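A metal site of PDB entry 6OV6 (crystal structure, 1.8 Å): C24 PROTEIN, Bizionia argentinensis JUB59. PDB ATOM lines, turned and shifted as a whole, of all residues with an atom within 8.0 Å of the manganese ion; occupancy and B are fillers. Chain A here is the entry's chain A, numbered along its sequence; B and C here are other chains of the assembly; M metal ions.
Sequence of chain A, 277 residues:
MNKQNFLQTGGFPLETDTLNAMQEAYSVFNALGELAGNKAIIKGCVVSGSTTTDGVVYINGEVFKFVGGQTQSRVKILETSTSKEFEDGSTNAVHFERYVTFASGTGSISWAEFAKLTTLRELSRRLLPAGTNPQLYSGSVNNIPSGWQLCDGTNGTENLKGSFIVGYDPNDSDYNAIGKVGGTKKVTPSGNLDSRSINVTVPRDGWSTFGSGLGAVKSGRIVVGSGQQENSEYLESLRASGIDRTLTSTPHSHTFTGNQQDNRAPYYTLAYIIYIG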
ATOM      1  N   LEU A 193     -27.775   0.548  28.602  1.00  0.00           N
ATOM      2  CA  LEU A 193     -27.046   1.560  27.823  1.00  0.00           C
ATOM      3  C   LEU A 193     -26.760   2.752  28.734  1.00  0.00           C
ATOM      4  O   LEU A 193     -27.579   3.080  29.599  1.00  0.00           O
ATOM      5  CB  LEU A 193     -27.917   2.043  26.640  1.00  0.00           C
ATOM      6  CG  LEU A 193     -28.140   1.099  25.426  1.00  0.00           C
ATOM      7  CD1 LEU A 193     -26.867   0.499  24.950  1.00  0.00           C
ATOM      8  CD2 LEU A 193     -29.092  -0.065  25.743  1.00  0.00           C
ATOM      9  N   ASP A 194     -25.632   3.419  28.495  1.00  0.00           N
ATOM     10  CA  ASP A 194     -25.309   4.611  29.299  1.00  0.00           C
ATOM     11  C   ASP A 194     -26.083   5.820  28.712  1.00  0.00           C
ATOM     12  O   ASP A 194     -26.741   5.678  27.672  1.00  0.00           O
ATOM     13  CB  ASP A 194     -23.787   4.831  29.382  1.00  0.00           C
ATOM     14  CG  ASP A 194     -23.061   5.085  28.083  1.00  0.00           C
ATOM     15  OD1 ASP A 194     -23.617   4.755  27.009  1.00  0.00           O
ATOM     16  OD2 ASP A 194     -21.949   5.621  28.130  1.00  0.00           O
ATOM     17  N   SER A 195     -26.082   6.969  29.437  1.00  0.00           N
ATOM     18  CA  SER A 195     -26.831   8.188  29.070  1.00  0.00           C
ATOM     19  C   SER A 195     -25.911   9.181  28.381  1.00  0.00           C
ATOM     20  O   SER A 195     -24.771   9.351  28.814  1.00  0.00           O
ATOM     21  CB  SER A 195     -27.432   8.858  30.304  1.00  0.00           C
ATOM     22  OG  SER A 195     -28.479   8.058  30.845  1.00  0.00           O
ATOM     23  N   ARG A 196     -26.388   9.816  27.276  1.00  0.00           N
ATOM     24  CA  ARG A 196     -25.578  10.778  26.533  1.00  0.00           C
ATOM     25  C   ARG A 196     -26.387  12.022  26.202  1.00  0.00           C
ATOM     26  O   ARG A 196     -27.610  11.955  26.054  1.00  0.00           O
ATOM     27  CB  ARG A 196     -25.033  10.173  25.224  1.00  0.00           C
ATOM     28  CG  ARG A 196     -24.248   8.858  25.389  1.00  0.00           C
ATOM     29  CD  ARG A 196     -22.740   9.053  25.496  1.00  0.00           C
ATOM     30  NE  ARG A 196     -22.044   7.780  25.782  1.00  0.00           N
ATOM     31  CZ  ARG A 196     -21.384   7.063  24.881  1.00  0.00           C
ATOM     32  NH1 ARG A 196     -21.278   7.485  23.623  1.00  0.00           N
ATOM     33  NH2 ARG A 196     -20.788   5.928  25.234  1.00  0.00           N
ATOM     34  N   ILE A 198     -26.287  15.637  23.570  1.00  0.00           N
ATOM     35  CA  ILE A 198     -25.784  16.097  22.281  1.00  0.00           C
ATOM     36  C   ILE A 198     -25.673  17.609  22.364  1.00  0.00           C
ATOM     37  O   ILE A 198     -26.253  18.223  23.260  1.00  0.00           O
ATOM     38  CB  ILE A 198     -26.596  15.613  21.029  1.00  0.00           C
ATOM     39  CG1 ILE A 198     -28.113  15.940  21.097  1.00  0.00           C
ATOM     40  CG2 ILE A 198     -26.360  14.123  20.711  1.00  0.00           C
ATOM     41  CD1 ILE A 198     -28.490  17.349  20.577  1.00  0.00           C
ATOM     42  N   HIS A 252     -30.002  11.335  27.546  1.00  0.00           N
ATOM     43  CA  HIS A 252     -30.980  10.318  27.171  1.00  0.00           C
ATOM     44  C   HIS A 252     -30.277   8.972  27.080  1.00  0.00           C
ATOM     45  O   HIS A 252     -29.060   8.913  26.849  1.00  0.00           O
ATOM     46  CB  HIS A 252     -31.651  10.625  25.813  1.00  0.00           C
ATOM     47  CG  HIS A 252     -30.802  10.236  24.645  1.00  0.00           C
ATOM     48  ND1 HIS A 252     -29.686  10.969  24.286  1.00  0.00           N
ATOM     49  CD2 HIS A 252     -30.914   9.170  23.820  1.00  0.00           C
ATOM     50  CE1 HIS A 252     -29.164  10.340  23.258  1.00  0.00           C
ATOM     51  NE2 HIS A 252     -29.860   9.243  22.950  1.00  0.00           N
ATOM     52  N   SER A 253     -31.050   7.907  27.219  1.00  0.00           N
ATOM     53  CA  SER A 253     -30.558   6.535  27.075  1.00  0.00           C
ATOM     54  C   SER A 253     -31.582   5.801  26.215  1.00  0.00           C
ATOM     55  O   SER A 253     -32.497   6.433  25.688  1.00  0.00           O
ATOM     56  CB  SER A 253     -30.433   5.871  28.447  1.00  0.00           C
ATOM     57  OG  SER A 253     -29.684   4.676  28.300  1.00  0.00           O
ATOM     58  N   HIS A 254     -31.439   4.463  26.055  1.00  0.00           N
ATOM     59  CA  HIS A 254     -32.412   3.646  25.315  1.00  0.00           C
ATOM     60  C   HIS A 254     -32.591   2.346  26.098  1.00  0.00           C
ATOM     61  O   HIS A 254     -31.718   2.012  26.885  1.00  0.00           O
ATOM     62  CB  HIS A 254     -31.964   3.317  23.887  1.00  0.00           C
ATOM     63  CG  HIS A 254     -31.696   4.527  23.026  1.00  0.00           C
ATOM     64  ND1 HIS A 254     -32.634   4.982  22.128  1.00  0.00           N
ATOM     65  CD2 HIS A 254     -30.604   5.315  22.972  1.00  0.00           C
ATOM     66  CE1 HIS A 254     -32.081   6.033  21.528  1.00  0.00           C
ATOM     67  NE2 HIS A 254     -30.870   6.294  22.037  1.00  0.00           N
ATOM     68  N   LEU B 193     -33.400  -1.500  20.181  1.00  0.00           N
ATOM     69  CA  LEU B 193     -33.436  -0.360  21.068  1.00  0.00           C
ATOM     70  C   LEU B 193     -34.729   0.392  20.802  1.00  0.00           C
ATOM     71  O   LEU B 193     -35.176   0.470  19.647  1.00  0.00           O
ATOM     72  CB  LEU B 193     -32.267   0.581  20.797  1.00  0.00           C
ATOM     73  CG  LEU B 193     -30.880   0.180  21.242  1.00  0.00           C
ATOM     74  CD1 LEU B 193     -30.025   1.367  21.216  1.00  0.00           C
ATOM     75  CD2 LEU B 193     -30.838  -0.338  22.651  1.00  0.00           C
ATOM     76  N   ASP B 194     -35.321   0.977  21.858  1.00  0.00           N
ATOM     77  CA  ASP B 194     -36.521   1.773  21.650  1.00  0.00           C
ATOM     78  C   ASP B 194     -36.089   3.130  21.066  1.00  0.00           C
ATOM     79  O   ASP B 194     -34.902   3.445  21.039  1.00  0.00           O
ATOM     80  CB  ASP B 194     -37.318   1.938  22.959  1.00  0.00           C
ATOM     81  CG  ASP B 194     -36.605   2.647  24.093  1.00  0.00           C
ATOM     82  OD1 ASP B 194     -35.373   2.769  24.033  1.00  0.00           O
ATOM     83  OD2 ASP B 194     -37.281   3.047  25.050  1.00  0.00           O
ATOM     84  N   SER B 195     -37.061   3.931  20.627  1.00  0.00           N
ATOM     85  CA  SER B 195     -36.788   5.251  20.075  1.00  0.00           C
ATOM     86  C   SER B 195     -36.916   6.302  21.183  1.00  0.00           C
ATOM     87  O   SER B 195     -37.847   6.252  21.976  1.00  0.00           O
ATOM     88  CB  SER B 195     -37.764   5.539  18.948  1.00  0.00           C
ATOM     89  OG  SER B 195     -37.478   4.696  17.853  1.00  0.00           O
ATOM     90  N   ARG B 196     -35.960   7.223  21.253  1.00  0.00           N
ATOM     91  CA  ARG B 196     -35.932   8.258  22.288  1.00  0.00           C
ATOM     92  C   ARG B 196     -35.657   9.624  21.685  1.00  0.00           C
ATOM     93  O   ARG B 196     -35.022   9.750  20.626  1.00  0.00           O
ATOM     94  CB  ARG B 196     -34.878   7.929  23.365  1.00  0.00           C
ATOM     95  CG  ARG B 196     -35.122   6.586  24.084  1.00  0.00           C
ATOM     96  CD  ARG B 196     -35.976   6.690  25.344  1.00  0.00           C
ATOM     97  NE  ARG B 196     -36.134   5.385  25.976  1.00  0.00           N
ATOM     98  CZ  ARG B 196     -35.558   5.010  27.114  1.00  0.00           C
ATOM     99  NH1 ARG B 196     -34.782   5.863  27.780  1.00  0.00           N
ATOM    100  NH2 ARG B 196     -35.766   3.800  27.612  1.00  0.00           N
ATOM    101  N   SER B 197     -36.091  10.657  22.380  1.00  0.00           N
ATOM    102  CA  SER B 197     -35.881  12.043  22.010  1.00  0.00           C
ATOM    103  C   SER B 197     -35.034  12.694  23.117  1.00  0.00           C
ATOM    104  O   SER B 197     -34.887  12.159  24.225  1.00  0.00           O
ATOM    105  CB  SER B 197     -37.236  12.745  21.962  1.00  0.00           C
ATOM    106  OG  SER B 197     -37.990  12.415  20.811  1.00  0.00           O
ATOM    107  N   ILE B 198     -34.435  13.846  22.804  1.00  0.00           N
ATOM    108  CA  ILE B 198     -33.738  14.674  23.794  1.00  0.00           C
ATOM    109  C   ILE B 198     -34.501  15.998  23.817  1.00  0.00           C
ATOM    110  O   ILE B 198     -35.282  16.250  22.919  1.00  0.00           O
ATOM    111  CB  ILE B 198     -32.205  14.899  23.556  1.00  0.00           C
ATOM    112  CG1 ILE B 198     -31.825  15.357  22.121  1.00  0.00           C
ATOM    113  CG2 ILE B 198     -31.401  13.680  23.995  1.00  0.00           C
ATOM    114  CD1 ILE B 198     -31.976  16.920  21.784  1.00  0.00           C
ATOM    115  N   HIS B 252     -35.154   8.998  17.829  1.00  0.00           N
ATOM    116  CA  HIS B 252     -34.071   8.277  17.137  1.00  0.00           C
ATOM    117  C   HIS B 252     -33.835   6.974  17.889  1.00  0.00           C
ATOM    118  O   HIS B 252     -34.138   6.859  19.076  1.00  0.00           O
ATOM    119  CB  HIS B 252     -32.785   9.088  17.071  1.00  0.00           C
ATOM    120  CG  HIS B 252     -32.002   9.057  18.347  1.00  0.00           C
ATOM    121  ND1 HIS B 252     -32.397   9.807  19.433  1.00  0.00           N
ATOM    122  CD2 HIS B 252     -30.918   8.326  18.697  1.00  0.00           C
ATOM    123  CE1 HIS B 252     -31.557   9.515  20.413  1.00  0.00           C
ATOM    124  NE2 HIS B 252     -30.646   8.621  20.020  1.00  0.00           N
ATOM    125  N   SER B 253     -33.229   6.021  17.217  1.00  0.00           N
ATOM    126  CA  SER B 253     -32.871   4.736  17.810  1.00  0.00           C
ATOM    127  C   SER B 253     -31.435   4.430  17.339  1.00  0.00           C
ATOM    128  O   SER B 253     -30.790   5.276  16.696  1.00  0.00           O
ATOM    129  CB  SER B 253     -33.838   3.663  17.314  1.00  0.00           C
ATOM    130  OG  SER B 253     -33.696   2.489  18.094  1.00  0.00           O
ATOM    131  N   HIS B 254     -30.913   3.236  17.661  1.00  0.00           N
ATOM    132  CA  HIS B 254     -29.582   2.799  17.232  1.00  0.00           C
ATOM    133  C   HIS B 254     -29.703   1.338  16.875  1.00  0.00           C
ATOM    134  O   HIS B 254     -30.647   0.679  17.321  1.00  0.00           O
ATOM    135  CB  HIS B 254     -28.524   2.945  18.340  1.00  0.00           C
ATOM    136  CG  HIS B 254     -28.344   4.333  18.858  1.00  0.00           C
ATOM    137  ND1 HIS B 254     -27.285   5.120  18.445  1.00  0.00           N
ATOM    138  CD2 HIS B 254     -29.097   5.021  19.738  1.00  0.00           C
ATOM    139  CE1 HIS B 254     -27.423   6.260  19.096  1.00  0.00           C
ATOM    140  NE2 HIS B 254     -28.509   6.256  19.873  1.00  0.00           N
ATOM    141  N   LEU C 193     -23.338  -0.273  19.464  1.00  0.00           N
ATOM    142  CA  LEU C 193     -24.402   0.525  18.865  1.00  0.00           C
ATOM    143  C   LEU C 193     -23.766   1.422  17.794  1.00  0.00           C
ATOM    144  O   LEU C 193     -22.640   1.879  17.964  1.00  0.00           O
ATOM    145  CB  LEU C 193     -25.041   1.430  19.905  1.00  0.00           C
ATOM    146  CG  LEU C 193     -25.955   0.806  20.951  1.00  0.00           C
ATOM    147  CD1 LEU C 193     -26.710   1.903  21.617  1.00  0.00           C
ATOM    148  CD2 LEU C 193     -26.945  -0.180  20.339  1.00  0.00           C
ATOM    149  N   ASP C 194     -24.481   1.657  16.703  1.00  0.00           N
ATOM    150  CA  ASP C 194     -23.984   2.580  15.675  1.00  0.00           C
ATOM    151  C   ASP C 194     -24.101   4.027  16.199  1.00  0.00           C
ATOM    152  O   ASP C 194     -24.765   4.267  17.215  1.00  0.00           O
ATOM    153  CB  ASP C 194     -24.747   2.398  14.355  1.00  0.00           C
ATOM    154  CG  ASP C 194     -26.237   2.675  14.386  1.00  0.00           C
ATOM    155  OD1 ASP C 194     -26.800   2.776  15.481  1.00  0.00           O
ATOM    156  OD2 ASP C 194     -26.849   2.775  13.302  1.00  0.00           O
ATOM    157  N   SER C 195     -23.442   4.975  15.516  1.00  0.00           N
ATOM    158  CA  SER C 195     -23.494   6.382  15.874  1.00  0.00           C
ATOM    159  C   SER C 195     -24.586   7.033  15.063  1.00  0.00           C
ATOM    160  O   SER C 195     -24.727   6.758  13.863  1.00  0.00           O
ATOM    161  CB  SER C 195     -22.149   7.051  15.580  1.00  0.00           C
ATOM    162  OG  SER C 195     -21.175   6.621  16.509  1.00  0.00           O
ATOM    163  N   ARG C 196     -25.394   7.889  15.721  1.00  0.00           N
ATOM    164  CA  ARG C 196     -26.493   8.583  15.065  1.00  0.00           C
ATOM    165  C   ARG C 196     -26.486  10.061  15.449  1.00  0.00           C
ATOM    166  O   ARG C 196     -26.067  10.426  16.544  1.00  0.00           O
ATOM    167  CB  ARG C 196     -27.866   7.969  15.447  1.00  0.00           C
ATOM    168  CG  ARG C 196     -28.001   6.474  15.168  1.00  0.00           C
ATOM    169  CD  ARG C 196     -28.656   6.179  13.851  1.00  0.00           C
ATOM    170  NE  ARG C 196     -28.772   4.738  13.637  1.00  0.00           N
ATOM    171  CZ  ARG C 196     -29.913   4.053  13.680  1.00  0.00           C
ATOM    172  NH1 ARG C 196     -31.068   4.680  13.912  1.00  0.00           N
ATOM    173  NH2 ARG C 196     -29.919   2.742  13.477  1.00  0.00           N
ATOM    174  N   SER C 197     -26.947  10.903  14.541  1.00  0.00           N
ATOM    175  CA  SER C 197     -27.088  12.336  14.795  1.00  0.00           C
ATOM    176  C   SER C 197     -28.558  12.593  15.104  1.00  0.00           C
ATOM    177  O   SER C 197     -29.431  11.894  14.605  1.00  0.00           O
ATOM    178  CB  SER C 197     -26.639  13.127  13.568  1.00  0.00           C
ATOM    179  OG  SER C 197     -25.229  13.256  13.621  1.00  0.00           O
ATOM    180  N   ILE C 198     -28.806  13.554  15.972  1.00  0.00           N
ATOM    181  CA  ILE C 198     -30.157  13.878  16.391  1.00  0.00           C
ATOM    182  C   ILE C 198     -30.550  15.197  15.712  1.00  0.00           C
ATOM    183  O   ILE C 198     -29.735  16.092  15.639  1.00  0.00           O
ATOM    184  CB  ILE C 198     -30.209  13.975  17.940  1.00  0.00           C
ATOM    185  CG1 ILE C 198     -29.971  12.587  18.607  1.00  0.00           C
ATOM    186  CG2 ILE C 198     -31.522  14.607  18.412  1.00  0.00           C
ATOM    187  CD1 ILE C 198     -29.900  12.583  20.292  1.00  0.00           C
ATOM    188  N   HIS C 252     -23.654  10.550  18.019  1.00  0.00           N
ATOM    189  CA  HIS C 252     -23.444   9.995  19.351  1.00  0.00           C
ATOM    190  C   HIS C 252     -23.765   8.513  19.297  1.00  0.00           C
ATOM    191  O   HIS C 252     -24.533   8.063  18.451  1.00  0.00           O
ATOM    192  CB  HIS C 252     -24.327  10.699  20.414  1.00  0.00           C
ATOM    193  CG  HIS C 252     -25.750  10.209  20.385  1.00  0.00           C
ATOM    194  ND1 HIS C 252     -26.616  10.572  19.375  1.00  0.00           N
ATOM    195  CD2 HIS C 252     -26.372   9.332  21.195  1.00  0.00           C
ATOM    196  CE1 HIS C 252     -27.738   9.913  19.614  1.00  0.00           C
ATOM    197  NE2 HIS C 252     -27.635   9.141  20.693  1.00  0.00           N
ATOM    198  N   SER C 253     -23.234   7.786  20.265  1.00  0.00           N
ATOM    199  CA  SER C 253     -23.528   6.350  20.424  1.00  0.00           C
ATOM    200  C   SER C 253     -23.792   6.122  21.892  1.00  0.00           C
ATOM    201  O   SER C 253     -23.817   7.090  22.663  1.00  0.00           O
ATOM    202  CB  SER C 253     -22.322   5.534  19.962  1.00  0.00           C
ATOM    203  OG  SER C 253     -22.700   4.179  19.787  1.00  0.00           O
ATOM    204  N   HIS C 254     -23.965   4.841  22.318  1.00  0.00           N
ATOM    205  CA  HIS C 254     -24.107   4.524  23.723  1.00  0.00           C
ATOM    206  C   HIS C 254     -23.294   3.255  23.946  1.00  0.00           C
ATOM    207  O   HIS C 254     -23.021   2.535  22.977  1.00  0.00           O
ATOM    208  CB  HIS C 254     -25.571   4.242  24.130  1.00  0.00           C
ATOM    209  CG  HIS C 254     -26.502   5.399  23.881  1.00  0.00           C
ATOM    210  ND1 HIS C 254     -26.861   6.281  24.892  1.00  0.00           N
ATOM    211  CD2 HIS C 254     -27.091   5.784  22.727  1.00  0.00           C
ATOM    212  CE1 HIS C 254     -27.680   7.155  24.329  1.00  0.00           C
ATOM    213  NE2 HIS C 254     -27.832   6.906  23.027  1.00  0.00           N
HETATM  214 MN    MN M   1     -29.234   7.692  21.405  1.00  0.00          MN
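The manganese ion is bound by NE2 of His 252 of chain B (2.2 Å), NE2 of His 254 of chain B (2.2 Å), NE2 of His 254 of chain A (2.2 Å), NE2 of His 252 of chain C (2.3 Å), NE2 of His 252 of chain A (2.3 Å) and NE2 of His 254 of chain C (2.3 Å). The manganese ion has six donor atoms within binding distance.
Six residues have an atom within 4 Å of the manganese ion: His 252 of chain A, His 254 of chain A, His 252 of chain B, His 254 of chain B, His 252 of chain C and His 254 of chain C. The nearest printed residue that does not touch the manganese ion is Ile 198 of chain C (5.1 Å).
N of Arg 196 of chain A sits at hydrogen-bond distance from O of His 252 of chain A, at 2.9 Å. The backbone carbonyl oxygen (O) of Asp 194 of chain B lies within hydrogen-bond range of a ring nitrogen (ND1) of His 254 of chain A, 2.9 Å away. The backbone NH of His 252 of chain C is in hydrogen-bond range of the backbone carbonyl oxygen of Arg 196 of chain C (2.8 Å). A ring nitrogen (ND1) of His 254 of chain B sits at hydrogen-bond distance from the backbone carbonyl oxygen (O) of Asp 194 of chain C (2.9 Å). The backbone NH of Arg 196 of chain B sits at hydrogen-bond distance from the backbone carbonyl oxygen of His 252 of chain B, 2.9 Å away. A ring nitrogen (ND1) of His 254 of chain C is in hydrogen-bond range of the backbone carbonyl oxygen (O) of Asp 194 of chain A (2.8 Å).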
